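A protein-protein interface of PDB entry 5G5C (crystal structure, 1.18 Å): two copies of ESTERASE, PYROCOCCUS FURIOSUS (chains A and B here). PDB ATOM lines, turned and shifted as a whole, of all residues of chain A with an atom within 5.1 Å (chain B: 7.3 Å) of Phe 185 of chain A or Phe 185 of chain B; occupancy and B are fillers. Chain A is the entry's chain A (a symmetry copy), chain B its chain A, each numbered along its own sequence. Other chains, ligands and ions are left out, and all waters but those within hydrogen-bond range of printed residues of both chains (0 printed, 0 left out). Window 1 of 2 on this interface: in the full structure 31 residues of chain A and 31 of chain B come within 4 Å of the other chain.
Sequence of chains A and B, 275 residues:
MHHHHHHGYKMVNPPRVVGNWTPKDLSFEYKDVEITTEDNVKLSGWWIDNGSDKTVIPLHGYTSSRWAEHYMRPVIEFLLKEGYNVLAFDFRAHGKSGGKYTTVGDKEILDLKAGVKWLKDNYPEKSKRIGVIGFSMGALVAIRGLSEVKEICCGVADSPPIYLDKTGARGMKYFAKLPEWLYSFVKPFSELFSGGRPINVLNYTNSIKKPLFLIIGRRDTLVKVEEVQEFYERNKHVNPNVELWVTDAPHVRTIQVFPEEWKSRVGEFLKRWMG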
ATOM      1  N   PRO A  15      -1.513 -17.214   4.844  1.00  0.00           N
ATOM      2  CA  PRO A  15      -0.836 -17.871   5.958  1.00  0.00           C
ATOM      3  C   PRO A  15      -0.430 -19.285   5.574  1.00  0.00           C
ATOM      4  O   PRO A  15      -1.072 -19.901   4.716  1.00  0.00           O
ATOM      5  CB  PRO A  15      -1.901 -17.891   7.048  1.00  0.00           C
ATOM      6  CG  PRO A  15      -2.830 -16.775   6.691  1.00  0.00           C
ATOM      7  CD  PRO A  15      -2.882 -16.811   5.199  1.00  0.00           C
ATOM      8  N   THR A  63      -6.114 -19.947   1.484  1.00  0.00           N
ATOM      9  CA  THR A  63      -5.577 -19.856   2.857  1.00  0.00           C
ATOM     10  C   THR A  63      -5.511 -21.199   3.592  1.00  0.00           C
ATOM     11  O   THR A  63      -5.079 -21.258   4.740  1.00  0.00           O
ATOM     12  CB  THR A  63      -6.359 -18.863   3.764  1.00  0.00           C
ATOM     13  OG1 THR A  63      -7.586 -19.445   4.204  1.00  0.00           O
ATOM     14  CG2 THR A  63      -6.614 -17.539   3.056  1.00  0.00           C
ATOM     15  N   TRP A 181      -7.817  -4.990  16.386  1.00  0.00           N
ATOM     16  CA  TRP A 181      -6.612  -5.767  16.110  1.00  0.00           C
ATOM     17  C   TRP A 181      -6.901  -6.967  15.205  1.00  0.00           C
ATOM     18  O   TRP A 181      -6.063  -7.363  14.399  1.00  0.00           O
ATOM     19  CB  TRP A 181      -5.943  -6.234  17.411  1.00  0.00           C
ATOM     20  CG  TRP A 181      -6.858  -6.883  18.414  1.00  0.00           C
ATOM     21  CD1 TRP A 181      -7.503  -6.271  19.452  1.00  0.00           C
ATOM     22  CD2 TRP A 181      -7.196  -8.275  18.498  1.00  0.00           C
ATOM     23  NE1 TRP A 181      -8.235  -7.189  20.163  1.00  0.00           N
ATOM     24  CE2 TRP A 181      -8.060  -8.427  19.600  1.00  0.00           C
ATOM     25  CE3 TRP A 181      -6.849  -9.403  17.748  1.00  0.00           C
ATOM     26  CZ2 TRP A 181      -8.596  -9.668  19.962  1.00  0.00           C
ATOM     27  CZ3 TRP A 181      -7.385 -10.636  18.111  1.00  0.00           C
ATOM     28  CH2 TRP A 181      -8.242 -10.753  19.212  1.00  0.00           C
ATOM     29  N   LEU A 182      -8.089  -7.543  15.324  1.00  0.00           N
ATOM     30  CA  LEU A 182      -8.425  -8.712  14.521  1.00  0.00           C
ATOM     31  C   LEU A 182      -8.731  -8.297  13.077  1.00  0.00           C
ATOM     32  O   LEU A 182      -8.510  -9.064  12.137  1.00  0.00           O
ATOM     33  CB  LEU A 182      -9.605  -9.461  15.145  1.00  0.00           C
ATOM     34  CG  LEU A 182      -9.925 -10.857  14.607  1.00  0.00           C
ATOM     35  CD1 LEU A 182      -8.676 -11.718  14.505  1.00  0.00           C
ATOM     36  CD2 LEU A 182     -10.974 -11.522  15.483  1.00  0.00           C
ATOM     37  N   TYR A 183      -9.203  -7.057  12.936  1.00  0.00           N
ATOM     38  CA  TYR A 183      -9.612  -6.446  11.667  1.00  0.00           C
ATOM     39  C   TYR A 183      -8.427  -6.213  10.751  1.00  0.00           C
ATOM     40  O   TYR A 183      -8.433  -6.643   9.602  1.00  0.00           O
ATOM     41  CB  TYR A 183     -10.325  -5.117  11.959  1.00  0.00           C
ATOM     42  CG  TYR A 183     -10.761  -4.285  10.774  1.00  0.00           C
ATOM     43  CD1 TYR A 183     -11.889  -4.621  10.032  1.00  0.00           C
ATOM     44  CD2 TYR A 183     -10.057  -3.143  10.419  1.00  0.00           C
ATOM     45  CE1 TYR A 183     -12.272  -3.858   8.957  1.00  0.00           C
ATOM     46  CE2 TYR A 183     -10.442  -2.377   9.356  1.00  0.00           C
ATOM     47  CZ  TYR A 183     -11.547  -2.741   8.625  1.00  0.00           C
ATOM     48  OH  TYR A 183     -11.948  -1.957   7.566  1.00  0.00           O
ATOM     49  N   SER A 184      -7.417  -5.511  11.259  1.00  0.00           N
ATOM     50  CA  SER A 184      -6.197  -5.258  10.501  1.00  0.00           C
ATOM     51  C   SER A 184      -5.488  -6.568  10.152  1.00  0.00           C
ATOM     52  O   SER A 184      -4.669  -6.617   9.236  1.00  0.00           O
ATOM     53  CB  SER A 184      -5.281  -4.330  11.294  1.00  0.00           C
ATOM     54  OG  SER A 184      -5.898  -3.065  11.470  1.00  0.00           O
ATOM     55  N   PHE A 185      -5.811  -7.635  10.880  1.00  0.00           N
ATOM     56  CA  PHE A 185      -5.275  -8.948  10.552  1.00  0.00           C
ATOM     57  C   PHE A 185      -5.973  -9.559   9.338  1.00  0.00           C
ATOM     58  O   PHE A 185      -5.316 -10.084   8.438  1.00  0.00           O
ATOM     59  CB  PHE A 185      -5.397  -9.909  11.736  1.00  0.00           C
ATOM     60  CG  PHE A 185      -4.917 -11.298  11.428  1.00  0.00           C
ATOM     61  CD1 PHE A 185      -3.565 -11.557  11.301  1.00  0.00           C
ATOM     62  CD2 PHE A 185      -5.813 -12.339  11.232  1.00  0.00           C
ATOM     63  CE1 PHE A 185      -3.108 -12.827  11.012  1.00  0.00           C
ATOM     64  CE2 PHE A 185      -5.362 -13.610  10.939  1.00  0.00           C
ATOM     65  CZ  PHE A 185      -4.005 -13.854  10.829  1.00  0.00           C
ATOM     66  N   VAL A 186      -7.299  -9.498   9.317  1.00  0.00           N
ATOM     67  CA  VAL A 186      -8.049 -10.168   8.260  1.00  0.00           C
ATOM     68  C   VAL A 186      -8.226  -9.322   7.005  1.00  0.00           C
ATOM     69  O   VAL A 186      -8.514  -9.857   5.942  1.00  0.00           O
ATOM     70  CB  VAL A 186      -9.453 -10.608   8.742  1.00  0.00           C
ATOM     71  CG1 VAL A 186      -9.350 -11.518   9.956  1.00  0.00           C
ATOM     72  CG2 VAL A 186     -10.322  -9.402   9.037  1.00  0.00           C
ATOM     73  N   LYS A 187      -8.058  -8.009   7.110  1.00  0.00           N
ATOM     74  CA  LYS A 187      -8.353  -7.159   5.958  1.00  0.00           C
ATOM     75  C   LYS A 187      -7.498  -7.352   4.702  1.00  0.00           C
ATOM     76  O   LYS A 187      -8.039  -7.319   3.598  1.00  0.00           O
ATOM     77  CB  LYS A 187      -8.281  -5.687   6.318  1.00  0.00           C
ATOM     78  CG  LYS A 187      -8.651  -4.825   5.166  1.00  0.00           C
ATOM     79  CD  LYS A 187      -8.622  -3.348   5.555  1.00  0.00           C
ATOM     80  CE  LYS A 187      -9.551  -2.545   4.637  1.00  0.00           C
ATOM     81  NZ  LYS A 187      -9.615  -1.060   4.919  1.00  0.00           N
ATOM     82  N   PRO A 188      -6.168  -7.514   4.849  1.00  0.00           N
ATOM     83  CA  PRO A 188      -5.366  -7.639   3.626  1.00  0.00           C
ATOM     84  C   PRO A 188      -5.816  -8.772   2.704  1.00  0.00           C
ATOM     85  O   PRO A 188      -5.742  -8.630   1.484  1.00  0.00           O
ATOM     86  CB  PRO A 188      -3.959  -7.913   4.162  1.00  0.00           C
ATOM     87  CG  PRO A 188      -3.939  -7.250   5.490  1.00  0.00           C
ATOM     88  CD  PRO A 188      -5.318  -7.432   6.051  1.00  0.00           C
ATOM     89  N   PHE A 189      -6.295  -9.868   3.283  1.00  0.00           N
ATOM     90  CA  PHE A 189      -6.694 -11.032   2.500  1.00  0.00           C
ATOM     91  C   PHE A 189      -8.041 -10.837   1.839  1.00  0.00           C
ATOM     92  O   PHE A 189      -8.375 -11.517   0.868  1.00  0.00           O
ATOM     93  CB  PHE A 189      -6.708 -12.269   3.383  1.00  0.00           C
ATOM     94  CG  PHE A 189      -5.356 -12.648   3.854  1.00  0.00           C
ATOM     95  CD1 PHE A 189      -4.550 -13.448   3.071  1.00  0.00           C
ATOM     96  CD2 PHE A 189      -4.864 -12.161   5.050  1.00  0.00           C
ATOM     97  CE1 PHE A 189      -3.293 -13.775   3.481  1.00  0.00           C
ATOM     98  CE2 PHE A 189      -3.601 -12.492   5.466  1.00  0.00           C
ATOM     99  CZ  PHE A 189      -2.816 -13.304   4.675  1.00  0.00           C
ATOM    100  N   VAL B  12       2.943 -23.003  12.060  1.00  0.00           N
ATOM    101  CA  VAL B  12       2.043 -21.954  11.600  1.00  0.00           C
ATOM    102  C   VAL B  12       2.819 -20.685  11.276  1.00  0.00           C
ATOM    103  O   VAL B  12       3.222 -19.947  12.178  1.00  0.00           O
ATOM    104  CB  VAL B  12       0.965 -21.633  12.656  1.00  0.00           C
ATOM    105  CG1 VAL B  12       0.080 -20.486  12.190  1.00  0.00           C
ATOM    106  CG2 VAL B  12       0.127 -22.864  12.950  1.00  0.00           C
ATOM    107  N   PRO B  14       3.112 -16.900  10.022  1.00  0.00           N
ATOM    108  CA  PRO B  14       2.311 -15.680   9.927  1.00  0.00           C
ATOM    109  C   PRO B  14       2.029 -15.310   8.483  1.00  0.00           C
ATOM    110  O   PRO B  14       2.766 -15.706   7.584  1.00  0.00           O
ATOM    111  CB  PRO B  14       3.185 -14.619  10.613  1.00  0.00           C
ATOM    112  CG  PRO B  14       4.562 -15.216  10.668  1.00  0.00           C
ATOM    113  CD  PRO B  14       4.347 -16.686  10.794  1.00  0.00           C
ATOM    114  N   PRO B  15       0.943 -14.575   8.250  1.00  0.00           N
ATOM    115  CA  PRO B  15       0.718 -14.045   6.909  1.00  0.00           C
ATOM    116  C   PRO B  15       1.810 -13.052   6.540  1.00  0.00           C
ATOM    117  O   PRO B  15       2.397 -12.419   7.426  1.00  0.00           O
ATOM    118  CB  PRO B  15      -0.630 -13.347   7.033  1.00  0.00           C
ATOM    119  CG  PRO B  15      -1.297 -14.014   8.193  1.00  0.00           C
ATOM    120  CD  PRO B  15      -0.181 -14.276   9.150  1.00  0.00           C
ATOM    121  N   VAL B  17       2.410  -9.635   4.838  1.00  0.00           N
ATOM    122  CA  VAL B  17       1.765  -8.432   4.352  1.00  0.00           C
ATOM    123  C   VAL B  17       2.823  -7.417   3.935  1.00  0.00           C
ATOM    124  O   VAL B  17       3.664  -7.015   4.738  1.00  0.00           O
ATOM    125  CB  VAL B  17       0.842  -7.833   5.423  1.00  0.00           C
ATOM    126  CG1 VAL B  17       0.241  -6.527   4.940  1.00  0.00           C
ATOM    127  CG2 VAL B  17      -0.248  -8.832   5.793  1.00  0.00           C
ATOM    128  N   TYR B  62       3.463  -9.065  15.966  1.00  0.00           N
ATOM    129  CA  TYR B  62       3.149 -10.386  15.430  1.00  0.00           C
ATOM    130  C   TYR B  62       2.068 -10.293  14.367  1.00  0.00           C
ATOM    131  O   TYR B  62       1.046  -9.647  14.587  1.00  0.00           O
ATOM    132  CB  TYR B  62       2.709 -11.295  16.577  1.00  0.00           C
ATOM    133  CG  TYR B  62       2.201 -12.663  16.182  1.00  0.00           C
ATOM    134  CD1 TYR B  62       3.002 -13.546  15.471  1.00  0.00           C
ATOM    135  CD2 TYR B  62       0.930 -13.090  16.559  1.00  0.00           C
ATOM    136  CE1 TYR B  62       2.544 -14.807  15.122  1.00  0.00           C
ATOM    137  CE2 TYR B  62       0.462 -14.352  16.216  1.00  0.00           C
ATOM    138  CZ  TYR B  62       1.276 -15.200  15.499  1.00  0.00           C
ATOM    139  OH  TYR B  62       0.811 -16.452  15.159  1.00  0.00           O
ATOM    140  N   THR B  63       2.331 -10.937  13.229  1.00  0.00           N
ATOM    141  CA  THR B  63       1.524 -10.953  11.990  1.00  0.00           C
ATOM    142  C   THR B  63       1.569  -9.642  11.200  1.00  0.00           C
ATOM    143  O   THR B  63       0.943  -9.528  10.149  1.00  0.00           O
ATOM    144  CB  THR B  63       0.028 -11.306  12.230  1.00  0.00           C
ATOM    145  OG1 THR B  63      -0.673 -10.180  12.761  1.00  0.00           O
ATOM    146  CG2 THR B  63      -0.124 -12.515  13.143  1.00  0.00           C
ATOM    147  N   SER B  64       2.322  -8.669  11.684  1.00  0.00           N
ATOM    148  CA  SER B  64       2.427  -7.367  11.030  1.00  0.00           C
ATOM    149  C   SER B  64       3.679  -7.320  10.141  1.00  0.00           C
ATOM    150  O   SER B  64       4.191  -8.361   9.750  1.00  0.00           O
ATOM    151  CB  SER B  64       2.446  -6.263  12.088  1.00  0.00           C
ATOM    152  OG  SER B  64       2.222  -4.981  11.532  1.00  0.00           O
ATOM    153  N   HIS B  70      -1.107   1.874  10.574  1.00  0.00           N
ATOM    154  CA  HIS B  70      -1.667   2.474  11.774  1.00  0.00           C
ATOM    155  C   HIS B  70      -0.626   2.743  12.858  1.00  0.00           C
ATOM    156  O   HIS B  70      -0.919   3.485  13.800  1.00  0.00           O
ATOM    157  CB  HIS B  70      -2.832   1.632  12.338  1.00  0.00           C
ATOM    158  CG  HIS B  70      -2.554   0.166  12.461  1.00  0.00           C
ATOM    159  ND1 HIS B  70      -2.289  -0.643  11.377  1.00  0.00           N
ATOM    160  CD2 HIS B  70      -2.564  -0.650  13.544  1.00  0.00           C
ATOM    161  CE1 HIS B  70      -2.116  -1.887  11.789  1.00  0.00           C
ATOM    162  NE2 HIS B  70      -2.279  -1.917  13.100  1.00  0.00           N
ATOM    163  N   PRO B 179     -18.292 -16.295  11.514  1.00  0.00           N
ATOM    164  CA  PRO B 179     -18.797 -17.444  10.754  1.00  0.00           C
ATOM    165  C   PRO B 179     -17.717 -18.528  10.651  1.00  0.00           C
ATOM    166  O   PRO B 179     -16.588 -18.232  10.760  1.00  0.00           O
ATOM    167  CB  PRO B 179     -19.153 -16.841   9.411  1.00  0.00           C
ATOM    168  CG  PRO B 179     -18.428 -15.561   9.345  1.00  0.00           C
ATOM    169  CD  PRO B 179     -18.262 -15.071  10.718  1.00  0.00           C
ATOM    170  N   GLU B 180     -18.101 -19.770  10.441  1.00  0.00           N
ATOM    171  CA  GLU B 180     -17.160 -20.890  10.567  1.00  0.00           C
ATOM    172  C   GLU B 180     -15.938 -20.802   9.649  1.00  0.00           C
ATOM    173  O   GLU B 180     -14.845 -21.221  10.034  1.00  0.00           O
ATOM    174  CB  GLU B 180     -17.882 -22.229  10.343  1.00  0.00           C
ATOM    175  CG  GLU B 180     -18.156 -22.616   8.897  1.00  0.00           C
ATOM    176  CD  GLU B 180     -19.178 -21.725   8.225  1.00  0.00           C
ATOM    177  OE1 GLU B 180     -20.210 -21.426   8.860  1.00  0.00           O
ATOM    178  OE2 GLU B 180     -18.950 -21.334   7.058  1.00  0.00           O
ATOM    179  N   TRP B 181     -16.095 -20.233   8.456  1.00  0.00           N
ATOM    180  CA  TRP B 181     -14.955 -20.114   7.552  1.00  0.00           C
ATOM    181  C   TRP B 181     -13.910 -19.129   8.076  1.00  0.00           C
ATOM    182  O   TRP B 181     -12.714 -19.304   7.858  1.00  0.00           O
ATOM    183  CB  TRP B 181     -15.406 -19.710   6.141  1.00  0.00           C
ATOM    184  CG  TRP B 181     -16.347 -18.538   6.072  1.00  0.00           C
ATOM    185  CD1 TRP B 181     -17.713 -18.585   6.047  1.00  0.00           C
ATOM    186  CD2 TRP B 181     -15.992 -17.151   5.980  1.00  0.00           C
ATOM    187  NE1 TRP B 181     -18.229 -17.315   5.964  1.00  0.00           N
ATOM    188  CE2 TRP B 181     -17.194 -16.418   5.917  1.00  0.00           C
ATOM    189  CE3 TRP B 181     -14.776 -16.463   5.942  1.00  0.00           C
ATOM    190  CZ2 TRP B 181     -17.212 -15.022   5.834  1.00  0.00           C
ATOM    191  CZ3 TRP B 181     -14.798 -15.073   5.860  1.00  0.00           C
ATOM    192  CH2 TRP B 181     -16.009 -14.373   5.801  1.00  0.00           C
ATOM    193  N   LEU B 182     -14.351 -18.093   8.778  1.00  0.00           N
ATOM    194  CA  LEU B 182     -13.420 -17.093   9.281  1.00  0.00           C
ATOM    195  C   LEU B 182     -12.658 -17.636  10.495  1.00  0.00           C
ATOM    196  O   LEU B 182     -11.512 -17.252  10.747  1.00  0.00           O
ATOM    197  CB  LEU B 182     -14.166 -15.801   9.626  1.00  0.00           C
ATOM    198  CG  LEU B 182     -13.330 -14.551   9.905  1.00  0.00           C
ATOM    199  CD1 LEU B 182     -12.265 -14.341   8.841  1.00  0.00           C
ATOM    200  CD2 LEU B 182     -14.237 -13.336  10.013  1.00  0.00           C
ATOM    201  N   TYR B 183     -13.311 -18.559  11.202  1.00  0.00           N
ATOM    202  CA  TYR B 183     -12.815 -19.195  12.428  1.00  0.00           C
ATOM    203  C   TYR B 183     -11.628 -20.094  12.150  1.00  0.00           C
ATOM    204  O   TYR B 183     -10.581 -19.957  12.775  1.00  0.00           O
ATOM    205  CB  TYR B 183     -13.954 -20.002  13.068  1.00  0.00           C
ATOM    206  CG  TYR B 183     -13.629 -20.803  14.308  1.00  0.00           C
ATOM    207  CD1 TYR B 183     -13.491 -20.189  15.549  1.00  0.00           C
ATOM    208  CD2 TYR B 183     -13.490 -22.182  14.239  1.00  0.00           C
ATOM    209  CE1 TYR B 183     -13.193 -20.927  16.668  1.00  0.00           C
ATOM    210  CE2 TYR B 183     -13.204 -22.921  15.351  1.00  0.00           C
ATOM    211  CZ  TYR B 183     -13.051 -22.289  16.562  1.00  0.00           C
ATOM    212  OH  TYR B 183     -12.783 -23.035  17.688  1.00  0.00           O
ATOM    213  N   SER B 184     -11.802 -21.031  11.222  1.00  0.00           N
ATOM    214  CA  SER B 184     -10.725 -21.931  10.823  1.00  0.00           C
ATOM    215  C   SER B 184      -9.553 -21.149  10.225  1.00  0.00           C
ATOM    216  O   SER B 184      -8.430 -21.648  10.164  1.00  0.00           O
ATOM    217  CB  SER B 184     -11.257 -22.967   9.837  1.00  0.00           C
ATOM    218  OG  SER B 184     -12.234 -23.784  10.463  1.00  0.00           O
ATOM    219  N   PHE B 185      -9.814 -19.919   9.792  1.00  0.00           N
ATOM    220  CA  PHE B 185      -8.743 -19.058   9.311  1.00  0.00           C
ATOM    221  C   PHE B 185      -7.918 -18.483  10.461  1.00  0.00           C
ATOM    222  O   PHE B 185      -6.688 -18.489  10.411  1.00  0.00           O
ATOM    223  CB  PHE B 185      -9.293 -17.907   8.465  1.00  0.00           C
ATOM    224  CG  PHE B 185      -8.233 -16.952   7.999  1.00  0.00           C
ATOM    225  CD1 PHE B 185      -7.350 -17.321   7.001  1.00  0.00           C
ATOM    226  CD2 PHE B 185      -8.095 -15.698   8.575  1.00  0.00           C
ATOM    227  CE1 PHE B 185      -6.367 -16.457   6.564  1.00  0.00           C
ATOM    228  CE2 PHE B 185      -7.111 -14.831   8.146  1.00  0.00           C
ATOM    229  CZ  PHE B 185      -6.245 -15.212   7.138  1.00  0.00           C
ATOM    230  N   VAL B 186      -8.593 -17.981  11.488  1.00  0.00           N
ATOM    231  CA  VAL B 186      -7.887 -17.297  12.568  1.00  0.00           C
ATOM    232  C   VAL B 186      -7.385 -18.236  13.660  1.00  0.00           C
ATOM    233  O   VAL B 186      -6.500 -17.869  14.422  1.00  0.00           O
ATOM    234  CB  VAL B 186      -8.768 -16.214  13.237  1.00  0.00           C
ATOM    235  CG1 VAL B 186      -9.250 -15.199  12.213  1.00  0.00           C
ATOM    236  CG2 VAL B 186      -9.936 -16.849  13.966  1.00  0.00           C
ATOM    237  N   LYS B 187      -7.934 -19.442  13.746  1.00  0.00           N
ATOM    238  CA  LYS B 187      -7.570 -20.310  14.864  1.00  0.00           C
ATOM    239  C   LYS B 187      -6.112 -20.768  14.955  1.00  0.00           C
ATOM    240  O   LYS B 187      -5.563 -20.803  16.056  1.00  0.00           O
ATOM    241  CB  LYS B 187      -8.428 -21.562  14.899  1.00  0.00           C
ATOM    242  CG  LYS B 187      -8.107 -22.409  16.076  1.00  0.00           C
ATOM    243  CD  LYS B 187      -9.011 -23.641  16.126  1.00  0.00           C
ATOM    244  CE  LYS B 187      -9.122 -24.152  17.568  1.00  0.00           C
ATOM    245  NZ  LYS B 187      -9.993 -25.374  17.757  1.00  0.00           N
ATOM    246  N   PRO B 188      -5.488 -21.156  13.825  1.00  0.00           N
ATOM    247  CA  PRO B 188      -4.110 -21.644  13.951  1.00  0.00           C
ATOM    248  C   PRO B 188      -3.161 -20.652  14.621  1.00  0.00           C
ATOM    249  O   PRO B 188      -2.262 -21.067  15.352  1.00  0.00           O
ATOM    250  CB  PRO B 188      -3.693 -21.882  12.498  1.00  0.00           C
ATOM    251  CG  PRO B 188      -4.967 -22.193  11.800  1.00  0.00           C
ATOM    252  CD  PRO B 188      -6.005 -21.332  12.455  1.00  0.00           C
ATOM    253  N   PHE B 189      -3.375 -19.361  14.391  1.00  0.00           N
ATOM    254  CA  PHE B 189      -2.492 -18.333  14.931  1.00  0.00           C
ATOM    255  C   PHE B 189      -2.750 -18.077  16.400  1.00  0.00           C
ATOM    256  O   PHE B 189      -1.896 -17.543  17.109  1.00  0.00           O
ATOM    257  CB  PHE B 189      -2.643 -17.049  14.131  1.00  0.00           C
ATOM    258  CG  PHE B 189      -2.162 -17.186  12.737  1.00  0.00           C
ATOM    259  CD1 PHE B 189      -0.829 -16.989  12.444  1.00  0.00           C
ATOM    260  CD2 PHE B 189      -3.024 -17.570  11.728  1.00  0.00           C
ATOM    261  CE1 PHE B 189      -0.371 -17.142  11.171  1.00  0.00           C
ATOM    262  CE2 PHE B 189      -2.566 -17.722  10.446  1.00  0.00           C
ATOM    263  CZ  PHE B 189      -1.233 -17.506  10.171  1.00  0.00           C
ATOM    264  N   SER B 190      -3.938 -18.456  16.846  1.00  0.00           N
ATOM    265  CA  SER B 190      -4.260 -18.428  18.260  1.00  0.00           C
ATOM    266  C   SER B 190      -3.495 -19.521  18.987  1.00  0.00           C
ATOM    267  O   SER B 190      -2.872 -19.279  20.020  1.00  0.00           O
ATOM    268  CB  SER B 190      -5.756 -18.614  18.469  1.00  0.00           C
ATOM    269  OG  SER B 190      -6.043 -18.945  19.814  1.00  0.00           O
ATOM    270  N   ARG B 253      -2.427   1.534  19.409  1.00  0.00           N
ATOM    271  CA  ARG B 253      -2.958   2.652  18.634  1.00  0.00           C
ATOM    272  C   ARG B 253      -2.920   4.008  19.329  1.00  0.00           C
ATOM    273  O   ARG B 253      -3.577   4.945  18.872  1.00  0.00           O
ATOM    274  CB  ARG B 253      -4.379   2.331  18.182  1.00  0.00           C
ATOM    275  CG  ARG B 253      -4.372   1.325  17.045  1.00  0.00           C
ATOM    276  CD  ARG B 253      -5.751   0.892  16.661  1.00  0.00           C
ATOM    277  NE  ARG B 253      -5.697  -0.298  15.820  1.00  0.00           N
ATOM    278  CZ  ARG B 253      -5.878  -0.297  14.506  1.00  0.00           C
ATOM    279  NH1 ARG B 253      -6.129   0.838  13.870  1.00  0.00           N
ATOM    280  NH2 ARG B 253      -5.816  -1.439  13.835  1.00  0.00           N
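Among the printed residues, pairs that only touch across the chains: Phe 189 of chain A with Pro 15 of chain B, Pro 15 of chain A with Phe 189 of chain B, Pro 15 of chain A with Pro 15 of chain B, Phe 185 of chain A with Phe 185 of chain B, Thr 63 of chain A with Phe 185 of chain B, Phe 185 of chain A with Thr 63 of chain B, Pro 15 of chain A with Phe 185 of chain B, Phe 185 of chain A with Pro 15 of chain B, Phe 189 of chain A with Phe 185 of chain B, Phe 185 of chain A with Phe 189 of chain B and Ser 184 of chain A with His 70 of chain B.
The side-chain hydroxyl of Ser 184 of chain A sits at hydrogen-bond distance from the guanidinium group of Arg 253 of chain B (2.9 Å).
Of chain B, only Pro 15, Thr 63, Phe 185 and Phe 189 come within 4 Å of Phe 185 of chain A.
Of chain A, only Pro 15, Thr 63, Phe 185 and Phe 189 come within 4 Å of Phe 185 of chain B.
Of the printed residues of chain A, His 70 of chain B touches Ser 184 (3.97 Å).
Printed residues of chain B within 4 Å of Ser 184 of chain A: His 70 and Arg 253.
Of the printed residues of chain A, Phe 189 of chain B touches Pro 15 (3.2 Å) and Phe 185 (3.9 Å).
Lys 187 of chain A touches none of the printed residues of chain B.
The nearest printed residue of chain B that does not touch Ser 184 of chain A is Val 17 of chain B (6.0 Å).
Of the 21 printed residues of chain B, 6 touch a printed residue of chain A.
Hydrophobic or aromatic side chains of chain B within 4 Å of the printed part of chain A: Pro 15, His 70, Phe 185 and Phe 189.
Along chain B the printed residues that touch a printed residue of chain A span positions 15 to 253.
Of the 11 printed residues of chain A, 5 touch a printed residue of chain B.
Hydrophobic or aromatic side chains of chain A that line the printed part of chain B: Pro 15, Phe 185 and Phe 189.
Pro 15 of chain A touches Phe 185 of chain B, and with the chains exchanged Phe 185 of chain A touches Pro 15 of chain B.
Pro 15 of chain A touches Phe 189 of chain B, and with the chains exchanged Phe 189 of chain A touches Pro 15 of chain B.
Thr 63 of chain A touches Phe 185 of chain B, and with the chains exchanged Phe 185 of chain A touches Thr 63 of chain B.
Phe 185 of chain A touches its own counterpart, Phe 185 of chain B.
Positions printed for both chains: 15, 63, 181, 182, 183, 184, 185, 186, 187, 188 and 189.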
